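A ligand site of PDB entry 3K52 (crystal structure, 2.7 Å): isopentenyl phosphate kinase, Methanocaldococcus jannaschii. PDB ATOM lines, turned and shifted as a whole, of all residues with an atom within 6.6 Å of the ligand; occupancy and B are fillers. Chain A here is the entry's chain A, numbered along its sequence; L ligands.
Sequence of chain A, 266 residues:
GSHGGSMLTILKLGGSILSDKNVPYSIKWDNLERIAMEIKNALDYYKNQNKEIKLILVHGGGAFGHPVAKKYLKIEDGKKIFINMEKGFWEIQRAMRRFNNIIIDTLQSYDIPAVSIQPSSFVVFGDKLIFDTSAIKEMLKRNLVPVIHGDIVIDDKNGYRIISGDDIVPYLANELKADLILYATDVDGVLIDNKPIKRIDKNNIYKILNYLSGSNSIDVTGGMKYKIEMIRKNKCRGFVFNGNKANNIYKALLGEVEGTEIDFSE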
ATOM      1  N   LYS A  12       5.202  10.601   9.447  1.00  0.00           N
ATOM      2  CA  LYS A  12       5.493  11.517   8.360  1.00  0.00           C
ATOM      3  C   LYS A  12       5.078  10.893   7.047  1.00  0.00           C
ATOM      4  O   LYS A  12       5.693   9.923   6.587  1.00  0.00           O
ATOM      5  CB  LYS A  12       6.983  11.873   8.348  1.00  0.00           C
ATOM      6  CG  LYS A  12       7.274  13.264   7.828  1.00  0.00           C
ATOM      7  CD  LYS A  12       7.139  13.340   6.328  1.00  0.00           C
ATOM      8  CE  LYS A  12       7.793  14.596   5.797  1.00  0.00           C
ATOM      9  NZ  LYS A  12       7.782  14.645   4.306  1.00  0.00           N
ATOM     10  N   LYS A  21       3.874  14.839  -7.535  1.00  0.00           N
ATOM     11  CA  LYS A  21       4.415  16.167  -7.786  1.00  0.00           C
ATOM     12  C   LYS A  21       4.416  16.529  -9.264  1.00  0.00           C
ATOM     13  O   LYS A  21       4.466  17.705  -9.633  1.00  0.00           O
ATOM     14  CB  LYS A  21       5.832  16.270  -7.225  1.00  0.00           C
ATOM     15  CG  LYS A  21       5.922  16.012  -5.726  1.00  0.00           C
ATOM     16  CD  LYS A  21       7.246  16.510  -5.175  1.00  0.00           C
ATOM     17  CE  LYS A  21       7.478  17.969  -5.526  1.00  0.00           C
ATOM     18  NZ  LYS A  21       8.760  18.476  -4.966  1.00  0.00           N
ATOM     19  N   VAL A  58       2.306  14.488   9.759  1.00  0.00           N
ATOM     20  CA  VAL A  58       2.924  15.561   8.997  1.00  0.00           C
ATOM     21  C   VAL A  58       2.880  15.183   7.533  1.00  0.00           C
ATOM     22  O   VAL A  58       3.148  14.039   7.178  1.00  0.00           O
ATOM     23  CB  VAL A  58       4.393  15.752   9.400  1.00  0.00           C
ATOM     24  CG1 VAL A  58       5.010  16.919   8.628  1.00  0.00           C
ATOM     25  CG2 VAL A  58       4.514  15.946  10.900  1.00  0.00           C
ATOM     26  N   HIS A  59       2.534  16.151   6.682  1.00  0.00           N
ATOM     27  CA  HIS A  59       2.617  15.938   5.238  1.00  0.00           C
ATOM     28  C   HIS A  59       3.278  17.115   4.525  1.00  0.00           C
ATOM     29  O   HIS A  59       3.230  18.255   4.998  1.00  0.00           O
ATOM     30  CB  HIS A  59       1.240  15.613   4.642  1.00  0.00           C
ATOM     31  CG  HIS A  59       0.275  16.759   4.658  1.00  0.00           C
ATOM     32  ND1 HIS A  59       0.081  17.582   3.568  1.00  0.00           N
ATOM     33  CD2 HIS A  59      -0.572  17.202   5.618  1.00  0.00           C
ATOM     34  CE1 HIS A  59      -0.840  18.485   3.860  1.00  0.00           C
ATOM     35  NE2 HIS A  59      -1.248  18.271   5.096  1.00  0.00           N
ATOM     36  N   GLY A  60       3.907  16.834   3.386  1.00  0.00           N
ATOM     37  CA  GLY A  60       4.576  17.851   2.588  1.00  0.00           C
ATOM     38  C   GLY A  60       3.609  18.535   1.640  1.00  0.00           C
ATOM     39  O   GLY A  60       2.392  18.443   1.821  1.00  0.00           O
ATOM     40  N   GLY A  61       4.150  19.197   0.627  1.00  0.00           N
ATOM     41  CA  GLY A  61       3.346  20.016  -0.280  1.00  0.00           C
ATOM     42  C   GLY A  61       2.785  19.242  -1.451  1.00  0.00           C
ATOM     43  O   GLY A  61       1.827  19.682  -2.086  1.00  0.00           O
ATOM     44  N   GLY A  62       3.370  18.094  -1.752  1.00  0.00           N
ATOM     45  CA  GLY A  62       2.919  17.310  -2.882  1.00  0.00           C
ATOM     46  C   GLY A  62       2.810  18.179  -4.127  1.00  0.00           C
ATOM     47  O   GLY A  62       3.633  19.066  -4.340  1.00  0.00           O
ATOM     48  N   PHE A  64       0.919  20.423  -4.671  1.00  0.00           N
ATOM     49  CA  PHE A  64       0.234  21.656  -4.303  1.00  0.00           C
ATOM     50  C   PHE A  64       1.226  22.745  -3.949  1.00  0.00           C
ATOM     51  O   PHE A  64       1.272  23.784  -4.606  1.00  0.00           O
ATOM     52  CB  PHE A  64      -0.716  21.409  -3.138  1.00  0.00           C
ATOM     53  CG  PHE A  64      -1.965  20.661  -3.517  1.00  0.00           C
ATOM     54  CD1 PHE A  64      -3.177  21.324  -3.612  1.00  0.00           C
ATOM     55  CD2 PHE A  64      -1.926  19.311  -3.786  1.00  0.00           C
ATOM     56  CE1 PHE A  64      -4.327  20.645  -3.971  1.00  0.00           C
ATOM     57  CE2 PHE A  64      -3.076  18.632  -4.144  1.00  0.00           C
ATOM     58  CZ  PHE A  64      -4.271  19.296  -4.239  1.00  0.00           C
ATOM     59  N   GLY A  65       2.037  22.512  -2.923  1.00  0.00           N
ATOM     60  CA  GLY A  65       2.966  23.517  -2.443  1.00  0.00           C
ATOM     61  C   GLY A  65       4.067  23.873  -3.419  1.00  0.00           C
ATOM     62  O   GLY A  65       4.262  25.041  -3.747  1.00  0.00           O
ATOM     63  N   HIS A  66       4.801  22.863  -3.888  1.00  0.00           N
ATOM     64  CA  HIS A  66       5.979  23.101  -4.717  1.00  0.00           C
ATOM     65  C   HIS A  66       5.648  23.846  -6.018  1.00  0.00           C
ATOM     66  O   HIS A  66       6.270  24.865  -6.326  1.00  0.00           O
ATOM     67  CB  HIS A  66       6.693  21.775  -5.006  1.00  0.00           C
ATOM     68  CG  HIS A  66       7.050  21.005  -3.778  1.00  0.00           C
ATOM     69  ND1 HIS A  66       8.258  21.167  -3.119  1.00  0.00           N
ATOM     70  CD2 HIS A  66       6.358  20.083  -3.067  1.00  0.00           C
ATOM     71  CE1 HIS A  66       8.295  20.367  -2.076  1.00  0.00           C
ATOM     72  NE2 HIS A  66       7.157  19.695  -2.014  1.00  0.00           N
ATOM     73  N   PRO A  67       4.674  23.335  -6.779  1.00  0.00           N
ATOM     74  CA  PRO A  67       4.331  23.943  -8.076  1.00  0.00           C
ATOM     75  C   PRO A  67       4.052  25.427  -7.944  1.00  0.00           C
ATOM     76  O   PRO A  67       4.556  26.231  -8.735  1.00  0.00           O
ATOM     77  CB  PRO A  67       3.058  23.204  -8.484  1.00  0.00           C
ATOM     78  CG  PRO A  67       3.124  21.895  -7.769  1.00  0.00           C
ATOM     79  CD  PRO A  67       3.830  22.178  -6.467  1.00  0.00           C
ATOM     80  N   ALA A  69       4.868  27.402  -5.314  1.00  0.00           N
ATOM     81  CA  ALA A  69       6.028  28.077  -4.738  1.00  0.00           C
ATOM     82  C   ALA A  69       7.048  28.446  -5.806  1.00  0.00           C
ATOM     83  O   ALA A  69       7.628  29.528  -5.774  1.00  0.00           O
ATOM     84  CB  ALA A  69       6.665  27.218  -3.659  1.00  0.00           C
ATOM     85  N   ILE A  92       0.625  30.367  -1.902  1.00  0.00           N
ATOM     86  CA  ILE A  92       1.174  29.123  -1.364  1.00  0.00           C
ATOM     87  C   ILE A  92       0.358  28.640  -0.169  1.00  0.00           C
ATOM     88  O   ILE A  92       0.079  27.453  -0.028  1.00  0.00           O
ATOM     89  CB  ILE A  92       2.645  29.300  -0.962  1.00  0.00           C
ATOM     90  CG1 ILE A  92       3.499  29.584  -2.201  1.00  0.00           C
ATOM     91  CG2 ILE A  92       3.162  28.073  -0.232  1.00  0.00           C
ATOM     92  CD1 ILE A  92       4.752  30.379  -1.911  1.00  0.00           C
ATOM     93  N   MET A  96      -1.684  25.001  -0.102  1.00  0.00           N
ATOM     94  CA  MET A  96      -1.451  24.111   1.041  1.00  0.00           C
ATOM     95  C   MET A  96      -2.735  23.896   1.848  1.00  0.00           C
ATOM     96  O   MET A  96      -3.044  22.770   2.239  1.00  0.00           O
ATOM     97  CB  MET A  96      -0.324  24.632   1.928  1.00  0.00           C
ATOM     98  CG  MET A  96       1.034  24.687   1.246  1.00  0.00           C
ATOM     99  SD  MET A  96       1.587  23.090   0.620  1.00  0.00           S
ATOM    100  CE  MET A  96       1.377  22.044   2.065  1.00  0.00           C
ATOM    101  N   HIS A 149       1.481  20.553   8.206  1.00  0.00           N
ATOM    102  CA  HIS A 149       1.909  20.436   6.828  1.00  0.00           C
ATOM    103  C   HIS A 149       3.046  21.390   6.492  1.00  0.00           C
ATOM    104  O   HIS A 149       3.225  22.409   7.157  1.00  0.00           O
ATOM    105  CB  HIS A 149       0.733  20.656   5.861  1.00  0.00           C
ATOM    106  CG  HIS A 149       0.111  22.010   5.973  1.00  0.00           C
ATOM    107  ND1 HIS A 149       0.643  23.131   5.356  1.00  0.00           N
ATOM    108  CD2 HIS A 149      -1.009  22.428   6.609  1.00  0.00           C
ATOM    109  CE1 HIS A 149      -0.120  24.171   5.611  1.00  0.00           C
ATOM    110  NE2 HIS A 149      -1.130  23.783   6.373  1.00  0.00           N
ATOM    111  N   GLY A 150       3.836  21.033   5.492  1.00  0.00           N
ATOM    112  CA  GLY A 150       4.821  21.957   4.955  1.00  0.00           C
ATOM    113  C   GLY A 150       4.112  23.226   4.530  1.00  0.00           C
ATOM    114  O   GLY A 150       2.937  23.205   4.143  1.00  0.00           O
ATOM    115  N   ASP A 151       4.810  24.348   4.604  1.00  0.00           N
ATOM    116  CA  ASP A 151       4.168  25.626   4.378  1.00  0.00           C
ATOM    117  C   ASP A 151       5.192  26.699   4.055  1.00  0.00           C
ATOM    118  O   ASP A 151       6.390  26.520   4.274  1.00  0.00           O
ATOM    119  CB  ASP A 151       3.390  26.025   5.629  1.00  0.00           C
ATOM    120  CG  ASP A 151       2.200  26.908   5.325  1.00  0.00           C
ATOM    121  OD1 ASP A 151       2.027  27.299   4.151  1.00  0.00           O
ATOM    122  OD2 ASP A 151       1.449  27.217   6.270  1.00  0.00           O
ATOM    123  N   ILE A 152       4.710  27.825   3.532  1.00  0.00           N
ATOM    124  CA  ILE A 152       5.531  29.028   3.422  1.00  0.00           C
ATOM    125  C   ILE A 152       5.588  29.712   4.787  1.00  0.00           C
ATOM    126  O   ILE A 152       4.628  29.663   5.544  1.00  0.00           O
ATOM    127  CB  ILE A 152       4.931  30.005   2.403  1.00  0.00           C
ATOM    128  CG1 ILE A 152       5.903  31.156   2.107  1.00  0.00           C
ATOM    129  CG2 ILE A 152       3.594  30.551   2.906  1.00  0.00           C
ATOM    130  CD1 ILE A 152       7.118  30.726   1.325  1.00  0.00           C
ATOM    131  N   ILE A 162      10.707  28.150   2.906  1.00  0.00           N
ATOM    132  CA  ILE A 162       9.784  27.020   2.880  1.00  0.00           C
ATOM    133  C   ILE A 162      10.107  26.085   4.031  1.00  0.00           C
ATOM    134  O   ILE A 162      11.234  25.619   4.162  1.00  0.00           O
ATOM    135  CB  ILE A 162       9.867  26.233   1.573  1.00  0.00           C
ATOM    136  CG1 ILE A 162       9.344  27.062   0.397  1.00  0.00           C
ATOM    137  CG2 ILE A 162       9.063  24.951   1.694  1.00  0.00           C
ATOM    138  CD1 ILE A 162       7.833  27.215   0.384  1.00  0.00           C
ATOM    139  N   ILE A 163       9.123  25.811   4.868  1.00  0.00           N
ATOM    140  CA  ILE A 163       9.292  24.851   5.954  1.00  0.00           C
ATOM    141  C   ILE A 163       8.654  23.516   5.551  1.00  0.00           C
ATOM    142  O   ILE A 163       7.469  23.451   5.237  1.00  0.00           O
ATOM    143  CB  ILE A 163       8.672  25.376   7.266  1.00  0.00           C
ATOM    144  CG1 ILE A 163       8.974  24.425   8.423  1.00  0.00           C
ATOM    145  CG2 ILE A 163       7.171  25.582   7.107  1.00  0.00           C
ATOM    146  CD1 ILE A 163       8.432  24.912   9.747  1.00  0.00           C
ATOM    147  N   SER A 164       9.455  22.462   5.557  1.00  0.00           N
ATOM    148  CA  SER A 164       8.977  21.159   5.101  1.00  0.00           C
ATOM    149  C   SER A 164       8.800  20.188   6.246  1.00  0.00           C
ATOM    150  O   SER A 164       9.095  20.501   7.394  1.00  0.00           O
ATOM    151  CB  SER A 164       9.941  20.562   4.073  1.00  0.00           C
ATOM    152  OG  SER A 164      11.130  20.140   4.702  1.00  0.00           O
ATOM    153  N   GLY A 165       8.301  18.997   5.918  1.00  0.00           N
ATOM    154  CA  GLY A 165       8.172  17.935   6.896  1.00  0.00           C
ATOM    155  C   GLY A 165       9.501  17.641   7.562  1.00  0.00           C
ATOM    156  O   GLY A 165       9.562  17.422   8.774  1.00  0.00           O
ATOM    157  N   ASP A 166      10.563  17.645   6.759  1.00  0.00           N
ATOM    158  CA  ASP A 166      11.917  17.429   7.270  1.00  0.00           C
ATOM    159  C   ASP A 166      12.284  18.409   8.374  1.00  0.00           C
ATOM    160  O   ASP A 166      12.904  18.022   9.373  1.00  0.00           O
ATOM    161  CB  ASP A 166      12.925  17.498   6.128  1.00  0.00           C
ATOM    162  CG  ASP A 166      12.928  16.243   5.279  1.00  0.00           C
ATOM    163  OD1 ASP A 166      13.154  16.342   4.054  1.00  0.00           O
ATOM    164  OD2 ASP A 166      12.698  15.132   5.828  1.00  0.00           O
ATOM    165  N   ILE A 168       9.959  20.089  10.130  1.00  0.00           N
ATOM    166  CA  ILE A 168       8.924  20.010  11.151  1.00  0.00           C
ATOM    167  C   ILE A 168       9.062  18.789  12.070  1.00  0.00           C
ATOM    168  O   ILE A 168       8.845  18.892  13.286  1.00  0.00           O
ATOM    169  CB  ILE A 168       7.525  19.988  10.517  1.00  0.00           C
ATOM    170  CG1 ILE A 168       7.243  21.317   9.800  1.00  0.00           C
ATOM    171  CG2 ILE A 168       6.459  19.697  11.566  1.00  0.00           C
ATOM    172  CD1 ILE A 168       6.021  21.295   8.919  1.00  0.00           C
HETATM  173  O1  LIG L   1       9.228  19.852   1.499  1.00  0.00           O
HETATM  174  C1  LIG L   1       6.591  21.693   0.872  1.00  0.00           C
HETATM  175  O2  LIG L   1       7.081  20.946   1.988  1.00  0.00           O
HETATM  176  P1  LIG L   1       7.779  19.520   1.757  1.00  0.00           P
HETATM  177  C2  LIG L   1       6.432  23.163   1.262  1.00  0.00           C
HETATM  178  O3  LIG L   1       7.525  18.775   3.049  1.00  0.00           O
HETATM  179  C3  LIG L   1       5.826  23.933   0.115  1.00  0.00           C
HETATM  180  O4  LIG L   1       7.081  18.948   0.548  1.00  0.00           O
HETATM  181  C4  LIG L   1       4.694  24.882   0.363  1.00  0.00           C
HETATM  182  C5  LIG L   1       6.296  23.779  -1.115  1.00  0.00           C
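An oxygen (O4) of the ligand is in hydrogen-bond range of a ring nitrogen (NE2) of His 66, at 2.7 Å. The backbone NH (N) of Gly 61 lies within hydrogen-bond range of an oxygen (O4) of the ligand (2.9 Å). The backbone NH of Gly 165 sits at hydrogen-bond distance from an oxygen (O3) of the ligand (3.0 Å).
The side-chain amino group (NZ) of Lys 21 lies close to a ring nitrogen (ND1) of His 66, at 3.3 Å. The side-chain hydroxyl (OG) of Ser 164 sits close to the backbone NH (N) of Asp 166. The backbone NH of Gly 65 lies close to the side-chain sulfur of Met 96. N of Gly 150 sits at hydrogen-bond distance from O of His 59 (2.9 Å). N of Asp 151 lies within hydrogen-bond range of O of Ile 163 (2.9 Å).
Gly 60 touches the ligand (CA to O3, 3.1 Å). Gly 65 touches the ligand. Ile 92 touches the ligand. Met 96 touches the ligand (SD to C4, 3.6 Å). Gly 150 touches the ligand. N of Asp 151 touches C2 of the ligand, at 3.9 Å. Ile 162 touches the ligand (CG2 to C2, 3.2 Å). Ser 164 touches the ligand. The nearest printed residue that does not touch the ligand is Ile 163 (4.1 Å).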
